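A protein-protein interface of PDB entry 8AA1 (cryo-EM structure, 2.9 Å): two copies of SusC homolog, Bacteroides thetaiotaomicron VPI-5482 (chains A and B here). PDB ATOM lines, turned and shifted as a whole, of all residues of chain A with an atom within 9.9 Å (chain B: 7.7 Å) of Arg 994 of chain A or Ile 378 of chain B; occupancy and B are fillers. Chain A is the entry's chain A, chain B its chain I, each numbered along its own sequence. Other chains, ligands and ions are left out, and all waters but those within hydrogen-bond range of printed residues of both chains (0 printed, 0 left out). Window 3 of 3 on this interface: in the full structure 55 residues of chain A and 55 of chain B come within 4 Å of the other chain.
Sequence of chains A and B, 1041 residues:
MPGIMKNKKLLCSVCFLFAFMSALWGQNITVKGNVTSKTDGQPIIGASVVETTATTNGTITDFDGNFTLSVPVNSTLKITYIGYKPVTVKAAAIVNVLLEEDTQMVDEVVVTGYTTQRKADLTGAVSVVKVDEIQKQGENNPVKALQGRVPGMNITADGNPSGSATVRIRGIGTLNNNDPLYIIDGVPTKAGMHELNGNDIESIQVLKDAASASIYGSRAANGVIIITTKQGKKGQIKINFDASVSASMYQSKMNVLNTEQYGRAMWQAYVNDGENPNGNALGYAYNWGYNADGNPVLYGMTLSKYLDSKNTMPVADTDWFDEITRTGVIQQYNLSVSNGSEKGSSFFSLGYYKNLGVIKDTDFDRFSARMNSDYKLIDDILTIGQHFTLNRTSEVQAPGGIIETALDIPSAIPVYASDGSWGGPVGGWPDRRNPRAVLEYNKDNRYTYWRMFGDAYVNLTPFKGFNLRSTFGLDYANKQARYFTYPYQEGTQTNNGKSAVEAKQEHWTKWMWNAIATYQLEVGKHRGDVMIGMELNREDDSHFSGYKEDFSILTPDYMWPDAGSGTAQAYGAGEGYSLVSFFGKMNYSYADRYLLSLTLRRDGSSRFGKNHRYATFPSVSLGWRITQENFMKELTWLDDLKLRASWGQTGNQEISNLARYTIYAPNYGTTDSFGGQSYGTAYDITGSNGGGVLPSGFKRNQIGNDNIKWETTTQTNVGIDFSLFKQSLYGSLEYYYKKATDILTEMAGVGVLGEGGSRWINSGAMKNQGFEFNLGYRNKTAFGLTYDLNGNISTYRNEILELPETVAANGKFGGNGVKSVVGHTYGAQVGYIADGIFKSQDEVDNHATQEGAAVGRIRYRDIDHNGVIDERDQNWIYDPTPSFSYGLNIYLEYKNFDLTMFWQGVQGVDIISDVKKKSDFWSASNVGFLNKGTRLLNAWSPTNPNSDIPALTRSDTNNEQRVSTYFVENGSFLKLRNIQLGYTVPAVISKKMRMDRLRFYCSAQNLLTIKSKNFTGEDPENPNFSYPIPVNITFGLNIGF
Among the printed residues, merely in contact across the chains: Ile 237 of chain A with Lys 376 of chain B, Arg 994 of chain A with Ile 378 of chain B, Ile 239 of chain A with Leu 377 of chain B, Ile 237 of chain A with Lys 343 of chain B and Ile 237 of chain A with Leu 377 of chain B.
No position is printed for both chains.
Of the 5 pairs that touch across the chains among the printed residues, none has its exchanged pair printed and touching as well.
The backbone carbonyl oxygen of Lys 343 of chain B sits at hydrogen-bond distance from the backbone NH of Lys 376 of chain B.
The backbone NH of Leu 377 of chain B sits at hydrogen-bond distance from the backbone carbonyl oxygen of Leu 382 of chain B, at 2.9 Å.
Of the 21 printed residues of chain A, 3 touch a printed residue of chain B.
Printed residues of chain B that touch a printed residue of chain A: Lys 343, Lys 376, Leu 377 and Ile 378.
Among the printed residues, no Asp or Glu carboxylate lies within 4 Å of a Lys or Arg side-chain nitrogen of the other chain.
Arg 994 of chain A touches just one residue of chain B: Ile 378 (3.4 Å).
Of the printed residues of chain A, Ile 378 of chain B touches Arg 994 (3.4 Å).
No residue of chain A comes within 4 Å of Asp 379 of chain B.
No residue of chain A comes within 4 Å of Ile 381 of chain B.
Printed residues of chain A within 4 Å of Lys 376 of chain B: Ile 237 (3.4 Å).
Of the printed residues of chain B, Ile 237 of chain A touches Lys 343 (3.6 Å), Lys 376 (3.4 Å) and Leu 377 (3.9 Å).
Of the printed residues of chain B, Ile 239 of chain A touches Leu 377.
Printed residues of chain A within 4 Å of Lys 343 of chain B: Ile 237 (3.6 Å).
The nearest printed residue of chain B that does not touch Ile 239 of chain A is Leu 382 of chain B (4.2 Å).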
ATOM      1  N   ILE A 237       8.378  -8.354   3.842  1.00  0.00           N
ATOM      2  CA  ILE A 237       8.020  -7.433   2.773  1.00  0.00           C
ATOM      3  C   ILE A 237       8.658  -6.082   3.069  1.00  0.00           C
ATOM      4  O   ILE A 237       8.765  -5.683   4.234  1.00  0.00           O
ATOM      5  CB  ILE A 237       6.491  -7.304   2.621  1.00  0.00           C
ATOM      6  CG1 ILE A 237       6.137  -6.619   1.301  1.00  0.00           C
ATOM      7  CG2 ILE A 237       5.870  -6.584   3.815  1.00  0.00           C
ATOM      8  CD1 ILE A 237       4.696  -6.794   0.889  1.00  0.00           C
ATOM      9  N   LYS A 238       9.109  -5.396   2.023  1.00  0.00           N
ATOM     10  CA  LYS A 238       9.675  -4.061   2.166  1.00  0.00           C
ATOM     11  C   LYS A 238       9.230  -3.184   1.005  1.00  0.00           C
ATOM     12  O   LYS A 238       9.099  -3.651  -0.126  1.00  0.00           O
ATOM     13  CB  LYS A 238      11.211  -4.084   2.238  1.00  0.00           C
ATOM     14  CG  LYS A 238      11.794  -4.651   3.527  1.00  0.00           C
ATOM     15  CD  LYS A 238      11.414  -3.783   4.722  1.00  0.00           C
ATOM     16  CE  LYS A 238      11.834  -4.414   6.040  1.00  0.00           C
ATOM     17  NZ  LYS A 238      11.985  -5.885   5.925  1.00  0.00           N
ATOM     18  N   ILE A 239       8.976  -1.912   1.296  1.00  0.00           N
ATOM     19  CA  ILE A 239       8.731  -0.919   0.256  1.00  0.00           C
ATOM     20  C   ILE A 239       9.584   0.308   0.547  1.00  0.00           C
ATOM     21  O   ILE A 239       9.636   0.792   1.683  1.00  0.00           O
ATOM     22  CB  ILE A 239       7.234  -0.555   0.138  1.00  0.00           C
ATOM     23  CG1 ILE A 239       7.019   0.481  -0.966  1.00  0.00           C
ATOM     24  CG2 ILE A 239       6.684  -0.052   1.455  1.00  0.00           C
ATOM     25  CD1 ILE A 239       5.575   0.904  -1.128  1.00  0.00           C
ATOM     26  N   VAL A 337       9.436  -2.506  -4.269  1.00  0.00           N
ATOM     27  CA  VAL A 337       8.756  -3.397  -3.336  1.00  0.00           C
ATOM     28  C   VAL A 337       9.381  -4.782  -3.455  1.00  0.00           C
ATOM     29  O   VAL A 337       9.652  -5.266  -4.560  1.00  0.00           O
ATOM     30  CB  VAL A 337       7.232  -3.420  -3.587  1.00  0.00           C
ATOM     31  CG1 VAL A 337       6.919  -3.865  -5.004  1.00  0.00           C
ATOM     32  CG2 VAL A 337       6.533  -4.309  -2.566  1.00  0.00           C
ATOM     33  N   VAL A 985      14.845  10.236  10.983  1.00  0.00           N
ATOM     34  CA  VAL A 985      13.795  10.509  11.969  1.00  0.00           C
ATOM     35  C   VAL A 985      13.857   9.457  13.067  1.00  0.00           C
ATOM     36  O   VAL A 985      14.086   8.267  12.771  1.00  0.00           O
ATOM     37  CB  VAL A 985      12.414  10.523  11.290  1.00  0.00           C
ATOM     38  CG1 VAL A 985      11.310  10.776  12.302  1.00  0.00           C
ATOM     39  CG2 VAL A 985      12.382  11.572  10.191  1.00  0.00           C
ATOM     40  N   PRO A 986      13.690   9.824  14.340  1.00  0.00           N
ATOM     41  CA  PRO A 986      13.717   8.816  15.405  1.00  0.00           C
ATOM     42  C   PRO A 986      12.638   7.761  15.206  1.00  0.00           C
ATOM     43  O   PRO A 986      11.569   8.027  14.654  1.00  0.00           O
ATOM     44  CB  PRO A 986      13.470   9.637  16.676  1.00  0.00           C
ATOM     45  CG  PRO A 986      13.970  10.998  16.336  1.00  0.00           C
ATOM     46  CD  PRO A 986      13.665  11.195  14.878  1.00  0.00           C
ATOM     47  N   ALA A 987      12.946   6.544  15.663  1.00  0.00           N
ATOM     48  CA  ALA A 987      12.096   5.394  15.372  1.00  0.00           C
ATOM     49  C   ALA A 987      10.685   5.563  15.919  1.00  0.00           C
ATOM     50  O   ALA A 987       9.730   5.055  15.322  1.00  0.00           O
ATOM     51  CB  ALA A 987      12.730   4.120  15.933  1.00  0.00           C
ATOM     52  N   VAL A 988      10.527   6.260  17.045  1.00  0.00           N
ATOM     53  CA  VAL A 988       9.202   6.406  17.639  1.00  0.00           C
ATOM     54  C   VAL A 988       8.287   7.232  16.737  1.00  0.00           C
ATOM     55  O   VAL A 988       7.124   6.873  16.517  1.00  0.00           O
ATOM     56  CB  VAL A 988       9.311   7.002  19.055  1.00  0.00           C
ATOM     57  CG1 VAL A 988       9.886   5.973  20.012  1.00  0.00           C
ATOM     58  CG2 VAL A 988      10.183   8.248  19.049  1.00  0.00           C
ATOM     59  N   ILE A 989       8.795   8.340  16.191  1.00  0.00           N
ATOM     60  CA  ILE A 989       7.981   9.172  15.308  1.00  0.00           C
ATOM     61  C   ILE A 989       7.626   8.412  14.037  1.00  0.00           C
ATOM     62  O   ILE A 989       6.485   8.468  13.559  1.00  0.00           O
ATOM     63  CB  ILE A 989       8.705  10.496  14.994  1.00  0.00           C
ATOM     64  CG1 ILE A 989       8.827  11.358  16.253  1.00  0.00           C
ATOM     65  CG2 ILE A 989       7.976  11.261  13.901  1.00  0.00           C
ATOM     66  CD1 ILE A 989      10.157  11.235  16.961  1.00  0.00           C
ATOM     67  N   SER A 990       8.596   7.692  13.469  1.00  0.00           N
ATOM     68  CA  SER A 990       8.335   6.924  12.255  1.00  0.00           C
ATOM     69  C   SER A 990       7.299   5.834  12.500  1.00  0.00           C
ATOM     70  O   SER A 990       6.418   5.605  11.663  1.00  0.00           O
ATOM     71  CB  SER A 990       9.638   6.326  11.727  1.00  0.00           C
ATOM     72  OG  SER A 990      10.194   5.419  12.661  1.00  0.00           O
ATOM     73  N   LYS A 991       7.389   5.147  13.643  1.00  0.00           N
ATOM     74  CA  LYS A 991       6.394   4.134  13.978  1.00  0.00           C
ATOM     75  C   LYS A 991       5.024   4.761  14.196  1.00  0.00           C
ATOM     76  O   LYS A 991       3.998   4.147  13.881  1.00  0.00           O
ATOM     77  CB  LYS A 991       6.833   3.352  15.215  1.00  0.00           C
ATOM     78  CG  LYS A 991       7.970   2.378  14.957  1.00  0.00           C
ATOM     79  CD  LYS A 991       7.609   1.392  13.860  1.00  0.00           C
ATOM     80  CE  LYS A 991       8.760   0.443  13.569  1.00  0.00           C
ATOM     81  NZ  LYS A 991       8.422  -0.520  12.484  1.00  0.00           N
ATOM     82  N   LYS A 992       4.987   5.979  14.743  1.00  0.00           N
ATOM     83  CA  LYS A 992       3.728   6.710  14.822  1.00  0.00           C
ATOM     84  C   LYS A 992       3.165   6.962  13.428  1.00  0.00           C
ATOM     85  O   LYS A 992       1.963   6.780  13.199  1.00  0.00           O
ATOM     86  CB  LYS A 992       3.947   8.025  15.583  1.00  0.00           C
ATOM     87  CG  LYS A 992       3.074   9.225  15.190  1.00  0.00           C
ATOM     88  CD  LYS A 992       1.577   8.968  15.351  1.00  0.00           C
ATOM     89  CE  LYS A 992       0.786  10.265  15.291  1.00  0.00           C
ATOM     90  NZ  LYS A 992      -0.583  10.056  14.744  1.00  0.00           N
ATOM     91  N   MET A 993       4.018   7.346  12.482  1.00  0.00           N
ATOM     92  CA  MET A 993       3.611   7.583  11.105  1.00  0.00           C
ATOM     93  C   MET A 993       3.610   6.311  10.263  1.00  0.00           C
ATOM     94  O   MET A 993       3.469   6.395   9.039  1.00  0.00           O
ATOM     95  CB  MET A 993       4.518   8.636  10.464  1.00  0.00           C
ATOM     96  CG  MET A 993       3.845   9.983  10.251  1.00  0.00           C
ATOM     97  SD  MET A 993       4.879  11.155   9.353  1.00  0.00           S
ATOM     98  CE  MET A 993       3.653  12.343   8.811  1.00  0.00           C
ATOM     99  N   ARG A 994       3.783   5.147  10.891  1.00  0.00           N
ATOM    100  CA  ARG A 994       3.732   3.814  10.291  1.00  0.00           C
ATOM    101  C   ARG A 994       4.898   3.529   9.351  1.00  0.00           C
ATOM    102  O   ARG A 994       4.973   2.423   8.801  1.00  0.00           O
ATOM    103  CB  ARG A 994       2.415   3.562   9.539  1.00  0.00           C
ATOM    104  CG  ARG A 994       1.958   2.111   9.552  1.00  0.00           C
ATOM    105  CD  ARG A 994       1.777   1.602  10.971  1.00  0.00           C
ATOM    106  NE  ARG A 994       1.430   0.187  11.002  1.00  0.00           N
ATOM    107  CZ  ARG A 994       0.188  -0.280  10.975  1.00  0.00           C
ATOM    108  NH1 ARG A 994      -0.855   0.531  10.915  1.00  0.00           N
ATOM    109  NH2 ARG A 994      -0.010  -1.595  11.009  1.00  0.00           N
ATOM    110  N   MET A 995       5.813   4.472   9.150  1.00  0.00           N
ATOM    111  CA  MET A 995       6.980   4.229   8.314  1.00  0.00           C
ATOM    112  C   MET A 995       8.057   3.512   9.117  1.00  0.00           C
ATOM    113  O   MET A 995       8.322   3.867  10.269  1.00  0.00           O
ATOM    114  CB  MET A 995       7.521   5.544   7.755  1.00  0.00           C
ATOM    115  CG  MET A 995       6.470   6.413   7.089  1.00  0.00           C
ATOM    116  SD  MET A 995       7.093   8.051   6.671  1.00  0.00           S
ATOM    117  CE  MET A 995       5.563   8.974   6.554  1.00  0.00           C
ATOM    118  N   ASP A 996       8.671   2.495   8.512  1.00  0.00           N
ATOM    119  CA  ASP A 996       9.756   1.789   9.183  1.00  0.00           C
ATOM    120  C   ASP A 996      11.044   2.602   9.194  1.00  0.00           C
ATOM    121  O   ASP A 996      11.877   2.419  10.089  1.00  0.00           O
ATOM    122  CB  ASP A 996       9.996   0.433   8.518  1.00  0.00           C
ATOM    123  N   ARG A 997      11.223   3.494   8.221  1.00  0.00           N
ATOM    124  CA  ARG A 997      12.431   4.305   8.140  1.00  0.00           C
ATOM    125  C   ARG A 997      12.143   5.541   7.304  1.00  0.00           C
ATOM    126  O   ARG A 997      11.734   5.423   6.145  1.00  0.00           O
ATOM    127  CB  ARG A 997      13.590   3.508   7.535  1.00  0.00           C
ATOM    128  CG  ARG A 997      14.812   4.344   7.197  1.00  0.00           C
ATOM    129  CD  ARG A 997      15.964   3.468   6.738  1.00  0.00           C
ATOM    130  NE  ARG A 997      17.063   4.251   6.187  1.00  0.00           N
ATOM    131  CZ  ARG A 997      17.227   4.505   4.896  1.00  0.00           C
ATOM    132  NH1 ARG A 997      16.376   4.051   3.990  1.00  0.00           N
ATOM    133  NH2 ARG A 997      18.270   5.230   4.505  1.00  0.00           N
ATOM    134  N   LEU A 998      12.355   6.716   7.890  1.00  0.00           N
ATOM    135  CA  LEU A 998      12.187   7.989   7.200  1.00  0.00           C
ATOM    136  C   LEU A 998      13.475   8.782   7.344  1.00  0.00           C
ATOM    137  O   LEU A 998      13.931   9.029   8.466  1.00  0.00           O
ATOM    138  CB  LEU A 998      11.002   8.775   7.765  1.00  0.00           C
ATOM    139  CG  LEU A 998      10.740  10.148   7.145  1.00  0.00           C
ATOM    140  CD1 LEU A 998      10.508  10.025   5.649  1.00  0.00           C
ATOM    141  CD2 LEU A 998       9.557  10.822   7.821  1.00  0.00           C
ATOM    142  N   ILE A1039      11.685   6.970   2.190  1.00  0.00           N
ATOM    143  CA  ILE A1039      10.579   6.494   3.011  1.00  0.00           C
ATOM    144  C   ILE A1039      10.564   4.975   2.952  1.00  0.00           C
ATOM    145  O   ILE A1039      10.643   4.390   1.866  1.00  0.00           O
ATOM    146  CB  ILE A1039       9.231   7.072   2.542  1.00  0.00           C
ATOM    147  CG1 ILE A1039       9.327   8.591   2.385  1.00  0.00           C
ATOM    148  CG2 ILE A1039       8.123   6.696   3.509  1.00  0.00           C
ATOM    149  CD1 ILE A1039       8.044   9.237   1.914  1.00  0.00           C
ATOM    150  N   GLY A1040      10.462   4.342   4.118  1.00  0.00           N
ATOM    151  CA  GLY A1040      10.508   2.897   4.211  1.00  0.00           C
ATOM    152  C   GLY A1040       9.221   2.282   4.716  1.00  0.00           C
ATOM    153  O   GLY A1040       9.252   1.398   5.576  1.00  0.00           O
ATOM    154  N   PHE A1041       8.089   2.763   4.203  1.00  0.00           N
ATOM    155  CA  PHE A1041       6.757   2.282   4.583  1.00  0.00           C
ATOM    156  C   PHE A1041       6.675   0.764   4.729  1.00  0.00           C
ATOM    157  O   PHE A1041       5.614   0.217   5.030  1.00  0.00           O
ATOM    158  CB  PHE A1041       5.724   2.743   3.552  1.00  0.00           C
ATOM    159  CG  PHE A1041       4.847   3.862   4.029  1.00  0.00           C
ATOM    160  CD1 PHE A1041       4.710   5.018   3.280  1.00  0.00           C
ATOM    161  CD2 PHE A1041       4.154   3.756   5.221  1.00  0.00           C
ATOM    162  CE1 PHE A1041       3.901   6.051   3.714  1.00  0.00           C
ATOM    163  CE2 PHE A1041       3.343   4.784   5.662  1.00  0.00           C
ATOM    164  CZ  PHE A1041       3.217   5.933   4.907  1.00  0.00           C
ATOM    165  N   LYS B 343      -0.444 -13.113   1.726  1.00  0.00           N
ATOM    166  CA  LYS B 343       0.231 -11.833   1.838  1.00  0.00           C
ATOM    167  C   LYS B 343       0.705 -11.284   0.489  1.00  0.00           C
ATOM    168  O   LYS B 343       1.071 -10.105   0.409  1.00  0.00           O
ATOM    169  CB  LYS B 343       1.373 -11.997   2.858  1.00  0.00           C
ATOM    170  CG  LYS B 343       2.512 -10.988   2.926  1.00  0.00           C
ATOM    171  CD  LYS B 343       3.824 -11.512   2.353  1.00  0.00           C
ATOM    172  CE  LYS B 343       4.703 -10.373   1.863  1.00  0.00           C
ATOM    173  NZ  LYS B 343       6.123 -10.802   1.689  1.00  0.00           N
ATOM    174  N   LYS B 376       0.787  -6.926  -0.823  1.00  0.00           N
ATOM    175  CA  LYS B 376      -0.060  -6.241   0.143  1.00  0.00           C
ATOM    176  C   LYS B 376       0.809  -5.781   1.306  1.00  0.00           C
ATOM    177  O   LYS B 376       1.499  -6.598   1.925  1.00  0.00           O
ATOM    178  CB  LYS B 376      -1.181  -7.156   0.632  1.00  0.00           C
ATOM    179  CG  LYS B 376      -1.999  -7.772  -0.487  1.00  0.00           C
ATOM    180  CD  LYS B 376      -3.021  -8.754   0.057  1.00  0.00           C
ATOM    181  CE  LYS B 376      -3.811  -9.402  -1.066  1.00  0.00           C
ATOM    182  NZ  LYS B 376      -4.564  -8.397  -1.863  1.00  0.00           N
ATOM    183  N   LEU B 377       0.777  -4.485   1.602  1.00  0.00           N
ATOM    184  CA  LEU B 377       1.589  -3.940   2.674  1.00  0.00           C
ATOM    185  C   LEU B 377       0.722  -3.661   3.901  1.00  0.00           C
ATOM    186  O   LEU B 377      -0.498  -3.843   3.886  1.00  0.00           O
ATOM    187  CB  LEU B 377       2.316  -2.684   2.197  1.00  0.00           C
ATOM    188  CG  LEU B 377       3.545  -3.003   1.344  1.00  0.00           C
ATOM    189  CD1 LEU B 377       3.678  -2.024   0.186  1.00  0.00           C
ATOM    190  CD2 LEU B 377       4.808  -3.036   2.190  1.00  0.00           C
ATOM    191  N   ILE B 378       1.373  -3.211   4.976  1.00  0.00           N
ATOM    192  CA  ILE B 378       0.727  -2.966   6.264  1.00  0.00           C
ATOM    193  C   ILE B 378      -0.056  -4.208   6.669  1.00  0.00           C
ATOM    194  O   ILE B 378       0.529  -5.258   6.960  1.00  0.00           O
ATOM    195  CB  ILE B 378      -0.178  -1.719   6.221  1.00  0.00           C
ATOM    196  CG1 ILE B 378       0.426  -0.640   5.318  1.00  0.00           C
ATOM    197  CG2 ILE B 378      -0.377  -1.158   7.620  1.00  0.00           C
ATOM    198  CD1 ILE B 378       1.706  -0.036   5.852  1.00  0.00           C
ATOM    199  N   ASP B 379      -1.383  -4.097   6.695  1.00  0.00           N
ATOM    200  CA  ASP B 379      -2.261  -5.244   6.886  1.00  0.00           C
ATOM    201  C   ASP B 379      -3.167  -5.471   5.687  1.00  0.00           C
ATOM    202  O   ASP B 379      -3.209  -6.582   5.145  1.00  0.00           O
ATOM    203  CB  ASP B 379      -3.105  -5.066   8.159  1.00  0.00           C
ATOM    204  CG  ASP B 379      -3.515  -3.626   8.390  1.00  0.00           C
ATOM    205  OD1 ASP B 379      -3.179  -2.768   7.547  1.00  0.00           O
ATOM    206  OD2 ASP B 379      -4.173  -3.351   9.416  1.00  0.00           O
ATOM    207  N   ASP B 380      -3.895  -4.441   5.257  1.00  0.00           N
ATOM    208  CA  ASP B 380      -4.692  -4.508   4.039  1.00  0.00           C
ATOM    209  C   ASP B 380      -4.529  -3.288   3.146  1.00  0.00           C
ATOM    210  O   ASP B 380      -4.988  -3.326   2.000  1.00  0.00           O
ATOM    211  CB  ASP B 380      -6.179  -4.683   4.376  1.00  0.00           C
ATOM    212  CG  ASP B 380      -6.505  -6.082   4.863  1.00  0.00           C
ATOM    213  OD1 ASP B 380      -6.006  -7.054   4.257  1.00  0.00           O
ATOM    214  OD2 ASP B 380      -7.260  -6.209   5.849  1.00  0.00           O
ATOM    215  N   ILE B 381      -3.901  -2.216   3.622  1.00  0.00           N
ATOM    216  CA  ILE B 381      -3.690  -1.028   2.808  1.00  0.00           C
ATOM    217  C   ILE B 381      -2.478  -1.243   1.905  1.00  0.00           C
ATOM    218  O   ILE B 381      -1.672  -2.153   2.112  1.00  0.00           O
ATOM    219  CB  ILE B 381      -3.512   0.207   3.709  1.00  0.00           C
ATOM    220  CG1 ILE B 381      -4.544   0.190   4.837  1.00  0.00           C
ATOM    221  CG2 ILE B 381      -3.698   1.493   2.925  1.00  0.00           C
ATOM    222  CD1 ILE B 381      -4.275   1.208   5.922  1.00  0.00           C
ATOM    223  N   LEU B 382      -2.353  -0.395   0.883  1.00  0.00           N
ATOM    224  CA  LEU B 382      -1.182  -0.373   0.003  1.00  0.00           C
ATOM    225  C   LEU B 382      -0.987  -1.726  -0.689  1.00  0.00           C
ATOM    226  O   LEU B 382      -0.073  -2.501  -0.389  1.00  0.00           O
ATOM    227  CB  LEU B 382       0.074   0.045   0.778  1.00  0.00           C
ATOM    228  CG  LEU B 382       1.157   0.774  -0.020  1.00  0.00           C
ATOM    229  CD1 LEU B 382       0.550   1.554  -1.176  1.00  0.00           C
ATOM    230  CD2 LEU B 382       1.957   1.695   0.886  1.00  0.00           C
ATOM    231  N   THR B 383      -1.929  -2.019  -1.582  1.00  0.00           N
ATOM    232  CA  THR B 383      -1.840  -3.173  -2.470  1.00  0.00           C
ATOM    233  C   THR B 383      -1.266  -2.702  -3.803  1.00  0.00           C
ATOM    234  O   THR B 383      -1.940  -2.005  -4.564  1.00  0.00           O
ATOM    235  CB  THR B 383      -3.206  -3.825  -2.662  1.00  0.00           C
ATOM    236  OG1 THR B 383      -3.711  -4.261  -1.393  1.00  0.00           O
ATOM    237  CG2 THR B 383      -3.100  -5.018  -3.597  1.00  0.00           C
ATOM    238  N   LEU B 460      -5.155   1.939  -2.311  1.00  0.00           N
ATOM    239  CA  LEU B 460      -5.092   2.431  -0.944  1.00  0.00           C
ATOM    240  C   LEU B 460      -6.469   2.317  -0.306  1.00  0.00           C
ATOM    241  O   LEU B 460      -7.482   2.628  -0.940  1.00  0.00           O
ATOM    242  CB  LEU B 460      -4.617   3.887  -0.911  1.00  0.00           C
ATOM    243  CG  LEU B 460      -4.145   4.453   0.428  1.00  0.00           C
ATOM    244  CD1 LEU B 460      -2.676   4.132   0.651  1.00  0.00           C
ATOM    245  CD2 LEU B 460      -4.384   5.952   0.489  1.00  0.00           C
